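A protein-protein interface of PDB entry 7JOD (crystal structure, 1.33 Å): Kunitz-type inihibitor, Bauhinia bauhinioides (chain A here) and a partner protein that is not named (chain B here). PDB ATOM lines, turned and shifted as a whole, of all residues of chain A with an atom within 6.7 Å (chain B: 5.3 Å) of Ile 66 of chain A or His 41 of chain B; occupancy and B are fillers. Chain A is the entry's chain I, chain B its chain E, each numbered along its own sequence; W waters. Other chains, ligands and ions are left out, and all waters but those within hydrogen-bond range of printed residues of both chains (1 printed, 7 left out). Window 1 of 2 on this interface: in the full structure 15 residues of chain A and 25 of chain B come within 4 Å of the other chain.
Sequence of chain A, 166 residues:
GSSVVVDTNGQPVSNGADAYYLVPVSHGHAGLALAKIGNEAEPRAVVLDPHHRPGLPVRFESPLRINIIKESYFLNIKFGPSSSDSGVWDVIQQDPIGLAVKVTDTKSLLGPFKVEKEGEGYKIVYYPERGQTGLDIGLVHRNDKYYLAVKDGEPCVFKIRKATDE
O of His 41 of chain B is in hydrogen-bond range of NZ of Lys 70 of chain A (3.3 Å).
The side-chain hydroxyl of Tyr 73 of chain A lies within hydrogen-bond range of the backbone carbonyl oxygen of His 41 of chain B.
The backbone carbonyl oxygen (O) of Phe 43 of chain B is in hydrogen-bond range of the side-chain amino group (NZ) of Lys 70 of chain A, at 2.8 Å.
ND2 of Asn 174 of chain B lies within hydrogen-bond range of O of Asn 15 of chain A (3.2 Å).
N of Gly 175 of chain B is in hydrogen-bond range of O of Arg 65 of chain A, 2.8 Å away.
O of Arg 65 of chain A sits close to OG of Ser 177 of chain B, at 2.9 Å.
The side-chain hydroxyl of Ser 177 of chain B is in hydrogen-bond range of the backbone NH of Ile 66 of chain A (3.2 Å).
The backbone carbonyl oxygen (O) of Ser 192 of chain B sits at hydrogen-bond distance from the backbone NH (N) of Arg 65 of chain A, 3.1 Å away.
Water W1 lies within hydrogen-bond range of the backbone carbonyl oxygen of Ala 40 of chain B (2.8 Å) and the side-chain amino group of Lys 70 of chain A (3.2 Å).
Hydrophobic or aromatic side chains of chain A within 4 Å of the printed part of chain B: Leu 64, Ile 66 and Tyr 73.
Of the 15 printed residues of chain B, 9 touch a printed residue of chain A.
Along chain B the printed residues that touch a printed residue of chain A span positions 25 to 192.
Among the printed residues, 20 pairs touch across the chains.
Among the printed residues, no Asp or Glu carboxylate lies within 4 Å of a Lys or Arg side-chain nitrogen of the other chain.
Printed residues of chain B within 4 Å of Ile 66 of chain A: Phe 25, Cys 26, His 41, Asn 174, Gly 175 and Ser 177.
His 41 of chain B touches four residues of chain A.
Of the printed residues of chain A, Phe 25 of chain B touches Ile 66 (3.4 Å) and Asn 67 (3.5 Å).
Of the printed residues of chain A, Ser 192 of chain B touches Leu 64 (3.6 Å) and Arg 65 (3.1 Å).
Of the printed residues of chain A, Val 191 of chain B touches Arg 65.
Printed residues of chain B within 4 Å of Arg 65 of chain A: Asn 174 (3.5 Å), Gly 175 (2.8 Å), Ser 177 (2.8 Å), Val 191 (3.8 Å) and Ser 192 (3.1 Å).
Printed residues of chain A within 4 Å of Gly 175 of chain B: Arg 65 and Ile 66.
Ser 72 of chain A touches none of the printed residues of chain B.
Cys 42 of chain B touches none of the printed residues of chain A.
The nearest printed residue of chain B that does not touch Ile 66 of chain A is Cys 42 of chain B (4.3 Å).
SG of Cys 26 of chain B forms a disulfide with SG of Cys 42 of chain B (2.0 Å).
The side-chain hydroxyl (OG) of Ser 192 of chain B is in hydrogen-bond range of the side-chain carboxylate (OD2) of Asp 86 of chain B, 2.7 Å away.
The backbone NH (N) of Gly 178 of chain B sits at hydrogen-bond distance from the backbone carbonyl oxygen (O) of Val 191 of chain B (2.9 Å).
The backbone NH of Gly 1 of chain A lies within hydrogen-bond range of the side-chain hydroxyl of Ser 72 of chain A, at 3.3 Å.
The backbone NH (N) of Asn 15 of chain A sits at hydrogen-bond distance from the backbone carbonyl oxygen (O) of Asn 67 of chain A, 3.5 Å away.
The backbone NH (N) of Leu 64 of chain A lies within hydrogen-bond range of the side-chain hydroxyl (OG) of Ser 62 of chain A.
Leu 64 of chain A touches His 41 of chain B.
Leu 64 of chain A touches Ser 192 of chain B.
Arg 65 of chain A touches Asn 174 of chain B.
Val 191 of chain B touches Arg 65 of chain A.
O of Phe 25 of chain B touches CG1 of Ile 66 of chain A (3.4 Å).
Cys 26 of chain B touches Ile 66 of chain A.
Ile 66 of chain A touches His 41 of chain B (CB to NE2, 3.95 Å).
CG of Asn 174 of chain B touches O of Ile 66 of chain A, at 3.5 Å.
CA of Ile 66 of chain A touches N of Gly 175 of chain B, 3.95 Å away.
ND2 of Asn 67 of chain A touches CA of Phe 25 of chain B, at 3.5 Å.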
ATOM      1  N   GLY A   1     -33.476 -20.104  20.154  1.00  0.00           N
ATOM      2  CA  GLY A   1     -34.830 -20.676  20.296  1.00  0.00           C
ATOM      3  C   GLY A   1     -34.779 -22.190  20.411  1.00  0.00           C
ATOM      4  O   GLY A   1     -33.715 -22.756  20.105  1.00  0.00           O
ATOM      5  N   SER A  14     -32.636 -30.577   7.182  1.00  0.00           N
ATOM      6  CA  SER A  14     -31.166 -30.706   7.284  1.00  0.00           C
ATOM      7  C   SER A  14     -30.460 -29.372   6.994  1.00  0.00           C
ATOM      8  O   SER A  14     -30.963 -28.511   6.281  1.00  0.00           O
ATOM      9  CB  SER A  14     -30.548 -31.826   6.552  1.00  0.00           C
ATOM     10  OG  SER A  14     -30.619 -31.672   5.199  1.00  0.00           O
ATOM     11  N   ASN A  15     -29.302 -29.243   7.641  1.00  0.00           N
ATOM     12  CA  ASN A  15     -28.377 -28.113   7.398  1.00  0.00           C
ATOM     13  C   ASN A  15     -27.558 -28.454   6.146  1.00  0.00           C
ATOM     14  O   ASN A  15     -26.550 -29.135   6.263  1.00  0.00           O
ATOM     15  CB  ASN A  15     -27.532 -27.857   8.643  1.00  0.00           C
ATOM     16  CG  ASN A  15     -26.599 -26.672   8.476  1.00  0.00           C
ATOM     17  OD1 ASN A  15     -26.692 -25.981   7.462  1.00  0.00           O
ATOM     18  ND2 ASN A  15     -25.785 -26.484   9.504  1.00  0.00           N
ATOM     19  N   SER A  62     -26.549 -23.085   7.451  1.00  0.00           N
ATOM     20  CA  SER A  62     -26.010 -22.359   8.606  1.00  0.00           C
ATOM     21  C   SER A  62     -24.569 -22.815   8.783  1.00  0.00           C
ATOM     22  O   SER A  62     -24.214 -24.002   8.623  1.00  0.00           O
ATOM     23  CB  SER A  62     -26.768 -22.720   9.868  1.00  0.00           C
ATOM     24  OG  SER A  62     -26.118 -22.303  11.061  1.00  0.00           O
ATOM     25  N   PRO A  63     -23.655 -21.902   9.208  1.00  0.00           N
ATOM     26  CA  PRO A  63     -22.291 -22.335   9.513  1.00  0.00           C
ATOM     27  C   PRO A  63     -22.099 -23.170  10.773  1.00  0.00           C
ATOM     28  O   PRO A  63     -21.068 -23.808  10.957  1.00  0.00           O
ATOM     29  CB  PRO A  63     -21.564 -20.985   9.622  1.00  0.00           C
ATOM     30  CG  PRO A  63     -22.593 -20.035  10.173  1.00  0.00           C
ATOM     31  CD  PRO A  63     -23.886 -20.458   9.446  1.00  0.00           C
ATOM     32  N   LEU A  64     -23.139 -23.169  11.609  1.00  0.00           N
ATOM     33  CA  LEU A  64     -23.118 -23.964  12.840  1.00  0.00           C
ATOM     34  C   LEU A  64     -22.914 -25.441  12.476  1.00  0.00           C
ATOM     35  O   LEU A  64     -23.521 -25.924  11.465  1.00  0.00           O
ATOM     36  CB  LEU A  64     -24.417 -23.763  13.611  1.00  0.00           C
ATOM     37  CG  LEU A  64     -24.730 -22.334  14.039  1.00  0.00           C
ATOM     38  CD1 LEU A  64     -26.158 -22.243  14.555  1.00  0.00           C
ATOM     39  CD2 LEU A  64     -23.738 -21.856  15.077  1.00  0.00           C
ATOM     40  N   ARG A  65     -22.150 -26.152  13.287  1.00  0.00           N
ATOM     41  CA  ARG A  65     -21.816 -27.567  12.970  1.00  0.00           C
ATOM     42  C   ARG A  65     -22.876 -28.550  13.483  1.00  0.00           C
ATOM     43  O   ARG A  65     -22.531 -29.645  13.986  1.00  0.00           O
ATOM     44  CB  ARG A  65     -20.359 -27.834  13.357  1.00  0.00           C
ATOM     45  CG  ARG A  65     -19.542 -27.613  12.098  1.00  0.00           C
ATOM     46  CD  ARG A  65     -18.149 -27.230  12.207  1.00  0.00           C
ATOM     47  NE  ARG A  65     -17.687 -27.188  10.835  1.00  0.00           N
ATOM     48  CZ  ARG A  65     -16.430 -27.191  10.562  1.00  0.00           C
ATOM     49  NH1 ARG A  65     -15.575 -27.197  11.580  1.00  0.00           N
ATOM     50  NH2 ARG A  65     -16.061 -27.158   9.295  1.00  0.00           N
ATOM     51  N   ILE A  66     -24.108 -28.165  13.277  1.00  0.00           N
ATOM     52  CA  ILE A  66     -25.303 -28.972  13.633  1.00  0.00           C
ATOM     53  C   ILE A  66     -25.952 -29.394  12.320  1.00  0.00           C
ATOM     54  O   ILE A  66     -25.739 -28.767  11.273  1.00  0.00           O
ATOM     55  CB  ILE A  66     -26.219 -28.123  14.538  1.00  0.00           C
ATOM     56  CG1 ILE A  66     -27.310 -28.973  15.190  1.00  0.00           C
ATOM     57  CG2 ILE A  66     -26.788 -26.912  13.790  1.00  0.00           C
ATOM     58  CD1 ILE A  66     -28.073 -28.269  16.277  1.00  0.00           C
ATOM     59  N   ASN A  67     -26.706 -30.487  12.419  1.00  0.00           N
ATOM     60  CA  ASN A  67     -27.280 -31.200  11.253  1.00  0.00           C
ATOM     61  C   ASN A  67     -28.762 -30.862  11.079  1.00  0.00           C
ATOM     62  O   ASN A  67     -29.400 -31.515  10.269  1.00  0.00           O
ATOM     63  CB  ASN A  67     -27.055 -32.708  11.347  1.00  0.00           C
ATOM     64  CG  ASN A  67     -27.620 -33.427  12.565  1.00  0.00           C
ATOM     65  OD1 ASN A  67     -27.309 -34.605  12.769  1.00  0.00           O
ATOM     66  ND2 ASN A  67     -28.475 -32.788  13.350  1.00  0.00           N
ATOM     67  N   ILE A  68     -29.296 -29.940  11.870  1.00  0.00           N
ATOM     68  CA  ILE A  68     -30.710 -29.504  11.807  1.00  0.00           C
ATOM     69  C   ILE A  68     -30.771 -27.985  11.770  1.00  0.00           C
ATOM     70  O   ILE A  68     -29.775 -27.329  12.065  1.00  0.00           O
ATOM     71  CB  ILE A  68     -31.520 -30.077  12.991  1.00  0.00           C
ATOM     72  CG1 ILE A  68     -30.999 -29.541  14.330  1.00  0.00           C
ATOM     73  CG2 ILE A  68     -31.529 -31.606  12.920  1.00  0.00           C
ATOM     74  CD1 ILE A  68     -31.868 -29.902  15.505  1.00  0.00           C
ATOM     75  N   ILE A  69     -31.918 -27.447  11.433  1.00  0.00           N
ATOM     76  CA  ILE A  69     -32.161 -25.995  11.320  1.00  0.00           C
ATOM     77  C   ILE A  69     -33.208 -25.584  12.345  1.00  0.00           C
ATOM     78  O   ILE A  69     -34.298 -26.226  12.407  1.00  0.00           O
ATOM     79  CB  ILE A  69     -32.584 -25.634   9.886  1.00  0.00           C
ATOM     80  CG1 ILE A  69     -31.449 -25.977   8.918  1.00  0.00           C
ATOM     81  CG2 ILE A  69     -33.066 -24.212   9.842  1.00  0.00           C
ATOM     82  CD1 ILE A  69     -30.208 -25.226   9.131  1.00  0.00           C
ATOM     83  N   LYS A  70     -32.931 -24.569  13.117  1.00  0.00           N
ATOM     84  CA  LYS A  70     -33.860 -23.917  14.035  1.00  0.00           C
ATOM     85  C   LYS A  70     -34.418 -22.622  13.437  1.00  0.00           C
ATOM     86  O   LYS A  70     -33.730 -21.938  12.653  1.00  0.00           O
ATOM     87  CB  LYS A  70     -33.242 -23.693  15.407  1.00  0.00           C
ATOM     88  CG  LYS A  70     -32.928 -24.943  16.237  1.00  0.00           C
ATOM     89  CD  LYS A  70     -32.293 -24.311  17.497  1.00  0.00           C
ATOM     90  CE  LYS A  70     -31.978 -25.110  18.701  1.00  0.00           C
ATOM     91  NZ  LYS A  70     -31.638 -24.075  19.713  1.00  0.00           N
ATOM     92  N   SER A  72     -34.542 -19.856  14.797  1.00  0.00           N
ATOM     93  CA  SER A  72     -33.695 -18.753  15.292  1.00  0.00           C
ATOM     94  C   SER A  72     -32.454 -18.552  14.436  1.00  0.00           C
ATOM     95  O   SER A  72     -31.780 -17.526  14.641  1.00  0.00           O
ATOM     96  CB  SER A  72     -33.328 -18.993  16.749  1.00  0.00           C
ATOM     97  OG  SER A  72     -32.664 -20.248  16.917  1.00  0.00           O
ATOM     98  N   TYR A  73     -32.073 -19.517  13.635  1.00  0.00           N
ATOM     99  CA  TYR A  73     -30.783 -19.472  12.918  1.00  0.00           C
ATOM    100  C   TYR A  73     -30.877 -18.531  11.721  1.00  0.00           C
ATOM    101  O   TYR A  73     -31.818 -18.561  10.911  1.00  0.00           O
ATOM    102  CB  TYR A  73     -30.384 -20.846  12.387  1.00  0.00           C
ATOM    103  CG  TYR A  73     -30.057 -21.921  13.403  1.00  0.00           C
ATOM    104  CD1 TYR A  73     -29.885 -21.672  14.748  1.00  0.00           C
ATOM    105  CD2 TYR A  73     -29.798 -23.214  12.967  1.00  0.00           C
ATOM    106  CE1 TYR A  73     -29.537 -22.676  15.641  1.00  0.00           C
ATOM    107  CE2 TYR A  73     -29.442 -24.228  13.845  1.00  0.00           C
ATOM    108  CZ  TYR A  73     -29.306 -23.960  15.190  1.00  0.00           C
ATOM    109  OH  TYR A  73     -28.965 -24.969  16.048  1.00  0.00           O
ATOM    110  N   PHE B  25     -28.229 -35.126  17.386  1.00  0.00           N
ATOM    111  CA  PHE B  25     -28.165 -33.798  16.728  1.00  0.00           C
ATOM    112  C   PHE B  25     -26.957 -32.986  17.205  1.00  0.00           C
ATOM    113  O   PHE B  25     -26.549 -32.085  16.456  1.00  0.00           O
ATOM    114  CB  PHE B  25     -29.463 -33.005  16.884  1.00  0.00           C
ATOM    115  CG  PHE B  25     -29.799 -32.565  18.280  1.00  0.00           C
ATOM    116  CD1 PHE B  25     -30.400 -33.441  19.173  1.00  0.00           C
ATOM    117  CD2 PHE B  25     -29.501 -31.297  18.732  1.00  0.00           C
ATOM    118  CE1 PHE B  25     -30.760 -33.014  20.433  1.00  0.00           C
ATOM    119  CE2 PHE B  25     -29.817 -30.889  20.004  1.00  0.00           C
ATOM    120  CZ  PHE B  25     -30.440 -31.752  20.863  1.00  0.00           C
ATOM    121  N   CYS B  26     -26.445 -33.218  18.411  1.00  0.00           N
ATOM    122  CA  CYS B  26     -25.269 -32.476  18.945  1.00  0.00           C
ATOM    123  C   CYS B  26     -24.541 -33.395  19.907  1.00  0.00           C
ATOM    124  O   CYS B  26     -25.103 -34.450  20.347  1.00  0.00           O
ATOM    125  CB  CYS B  26     -25.687 -31.211  19.732  1.00  0.00           C
ATOM    126  SG  CYS B  26     -26.109 -29.784  18.692  1.00  0.00           S
ATOM    127  N   ALA B  39     -22.782 -26.593  23.163  1.00  0.00           N
ATOM    128  CA  ALA B  39     -22.929 -25.293  22.463  1.00  0.00           C
ATOM    129  C   ALA B  39     -24.306 -24.724  22.746  1.00  0.00           C
ATOM    130  O   ALA B  39     -25.320 -25.491  22.774  1.00  0.00           O
ATOM    131  CB  ALA B  39     -22.736 -25.484  20.983  1.00  0.00           C
ATOM    132  N   ALA B  40     -24.449 -23.432  22.949  1.00  0.00           N
ATOM    133  CA  ALA B  40     -25.758 -22.789  23.148  1.00  0.00           C
ATOM    134  C   ALA B  40     -26.653 -22.942  21.923  1.00  0.00           C
ATOM    135  O   ALA B  40     -27.885 -22.938  22.112  1.00  0.00           O
ATOM    136  CB  ALA B  40     -25.578 -21.326  23.484  1.00  0.00           C
ATOM    137  N   HIS B  41     -26.126 -23.083  20.724  1.00  0.00           N
ATOM    138  CA  HIS B  41     -26.982 -23.239  19.524  1.00  0.00           C
ATOM    139  C   HIS B  41     -27.674 -24.613  19.561  1.00  0.00           C
ATOM    140  O   HIS B  41     -28.590 -24.788  18.744  1.00  0.00           O
ATOM    141  CB  HIS B  41     -26.240 -22.980  18.231  1.00  0.00           C
ATOM    142  CG  HIS B  41     -25.246 -23.990  17.815  1.00  0.00           C
ATOM    143  ND1 HIS B  41     -23.881 -23.885  18.039  1.00  0.00           N
ATOM    144  CD2 HIS B  41     -25.385 -25.153  17.132  1.00  0.00           C
ATOM    145  CE1 HIS B  41     -23.267 -24.925  17.484  1.00  0.00           C
ATOM    146  NE2 HIS B  41     -24.172 -25.730  16.924  1.00  0.00           N
ATOM    147  N   CYS B  42     -27.260 -25.539  20.428  1.00  0.00           N
ATOM    148  CA  CYS B  42     -27.901 -26.864  20.569  1.00  0.00           C
ATOM    149  C   CYS B  42     -29.069 -26.833  21.570  1.00  0.00           C
ATOM    150  O   CYS B  42     -29.634 -27.909  21.869  1.00  0.00           O
ATOM    151  CB  CYS B  42     -26.849 -27.893  20.996  1.00  0.00           C
ATOM    152  SG  CYS B  42     -25.545 -28.154  19.784  1.00  0.00           S
ATOM    153  N   PHE B  43     -29.435 -25.678  22.130  1.00  0.00           N
ATOM    154  CA  PHE B  43     -30.492 -25.542  23.155  1.00  0.00           C
ATOM    155  C   PHE B  43     -31.768 -26.252  22.697  1.00  0.00           C
ATOM    156  O   PHE B  43     -32.225 -26.062  21.575  1.00  0.00           O
ATOM    157  CB  PHE B  43     -30.757 -24.069  23.471  1.00  0.00           C
ATOM    158  CG  PHE B  43     -31.904 -23.890  24.412  1.00  0.00           C
ATOM    159  CD1 PHE B  43     -31.706 -23.925  25.772  1.00  0.00           C
ATOM    160  CD2 PHE B  43     -33.187 -23.756  23.897  1.00  0.00           C
ATOM    161  CE1 PHE B  43     -32.784 -23.793  26.634  1.00  0.00           C
ATOM    162  CE2 PHE B  43     -34.264 -23.667  24.753  1.00  0.00           C
ATOM    163  CZ  PHE B  43     -34.061 -23.681  26.112  1.00  0.00           C
ATOM    164  N   TYR B  78     -24.659 -15.087  24.801  1.00  0.00           N
ATOM    165  CA  TYR B  78     -24.751 -15.902  23.583  1.00  0.00           C
ATOM    166  C   TYR B  78     -25.322 -15.088  22.426  1.00  0.00           C
ATOM    167  O   TYR B  78     -26.402 -14.469  22.534  1.00  0.00           O
ATOM    168  CB  TYR B  78     -25.573 -17.169  23.851  1.00  0.00           C
ATOM    169  CG  TYR B  78     -25.867 -17.905  22.577  1.00  0.00           C
ATOM    170  CD1 TYR B  78     -24.856 -18.288  21.692  1.00  0.00           C
ATOM    171  CD2 TYR B  78     -27.177 -18.246  22.263  1.00  0.00           C
ATOM    172  CE1 TYR B  78     -25.140 -18.930  20.503  1.00  0.00           C
ATOM    173  CE2 TYR B  78     -27.477 -18.862  21.081  1.00  0.00           C
ATOM    174  CZ  TYR B  78     -26.476 -19.206  20.201  1.00  0.00           C
ATOM    175  OH  TYR B  78     -26.830 -19.831  19.068  1.00  0.00           O
ATOM    176  N   ASP B  86     -20.707 -19.093  22.589  1.00  0.00           N
ATOM    177  CA  ASP B  86     -21.534 -20.259  22.190  1.00  0.00           C
ATOM    178  C   ASP B  86     -21.344 -21.415  23.179  1.00  0.00           C
ATOM    179  O   ASP B  86     -20.645 -22.411  22.880  1.00  0.00           O
ATOM    180  CB  ASP B  86     -21.239 -20.674  20.752  1.00  0.00           C
ATOM    181  CG  ASP B  86     -22.190 -21.713  20.170  1.00  0.00           C
ATOM    182  OD1 ASP B  86     -23.239 -21.974  20.833  1.00  0.00           O
ATOM    183  OD2 ASP B  86     -21.927 -22.172  19.041  1.00  0.00           O
ATOM    184  N   ASN B 174     -20.738 -31.319  10.419  1.00  0.00           N
ATOM    185  CA  ASN B 174     -22.137 -31.214  10.893  1.00  0.00           C
ATOM    186  C   ASN B 174     -22.508 -32.426  11.747  1.00  0.00           C
ATOM    187  O   ASN B 174     -22.316 -33.551  11.268  1.00  0.00           O
ATOM    188  CB  ASN B 174     -23.098 -31.089   9.717  1.00  0.00           C
ATOM    189  CG  ASN B 174     -23.100 -29.694   9.136  1.00  0.00           C
ATOM    190  OD1 ASN B 174     -22.383 -28.827   9.643  1.00  0.00           O
ATOM    191  ND2 ASN B 174     -23.958 -29.450   8.162  1.00  0.00           N
ATOM    192  N   GLY B 175     -23.079 -32.165  12.929  1.00  0.00           N
ATOM    193  CA  GLY B 175     -23.388 -33.192  13.944  1.00  0.00           C
ATOM    194  C   GLY B 175     -22.325 -33.283  15.032  1.00  0.00           C
ATOM    195  O   GLY B 175     -22.525 -33.951  16.045  1.00  0.00           O
ATOM    196  N   SER B 177     -21.171 -30.420  16.533  1.00  0.00           N
ATOM    197  CA  SER B 177     -21.456 -29.268  17.424  1.00  0.00           C
ATOM    198  C   SER B 177     -21.508 -29.678  18.874  1.00  0.00           C
ATOM    199  O   SER B 177     -22.240 -30.667  19.170  1.00  0.00           O
ATOM    200  CB  SER B 177     -22.767 -28.561  17.056  1.00  0.00           C
ATOM    201  OG  SER B 177     -22.536 -27.584  16.038  1.00  0.00           O
ATOM    202  N   GLY B 178     -20.933 -28.924  19.781  1.00  0.00           N
ATOM    203  CA  GLY B 178     -21.046 -29.116  21.218  1.00  0.00           C
ATOM    204  C   GLY B 178     -20.058 -30.106  21.778  1.00  0.00           C
ATOM    205  O   GLY B 178     -19.951 -30.170  23.009  1.00  0.00           O
ATOM    206  N   VAL B 191     -16.879 -27.699  19.749  1.00  0.00           N
ATOM    207  CA  VAL B 191     -17.166 -27.514  18.324  1.00  0.00           C
ATOM    208  C   VAL B 191     -18.292 -26.506  18.184  1.00  0.00           C
ATOM    209  O   VAL B 191     -19.376 -26.665  18.773  1.00  0.00           O
ATOM    210  CB  VAL B 191     -17.560 -28.855  17.654  1.00  0.00           C
ATOM    211  CG1 VAL B 191     -17.942 -28.629  16.203  1.00  0.00           C
ATOM    212  CG2 VAL B 191     -16.462 -29.882  17.772  1.00  0.00           C
ATOM    213  N   SER B 192     -18.079 -25.449  17.379  1.00  0.00           N
ATOM    214  CA  SER B 192     -19.086 -24.380  17.214  1.00  0.00           C
ATOM    215  C   SER B 192     -19.542 -24.213  15.783  1.00  0.00           C
ATOM    216  O   SER B 192     -20.698 -24.496  15.441  1.00  0.00           O
ATOM    217  CB  SER B 192     -18.584 -23.074  17.861  1.00  0.00           C
ATOM    218  OG  SER B 192     -19.541 -22.025  17.768  1.00  0.00           O
HETATM  219  O   HOH W   1     -30.057 -21.625  21.023  1.00  0.00           O
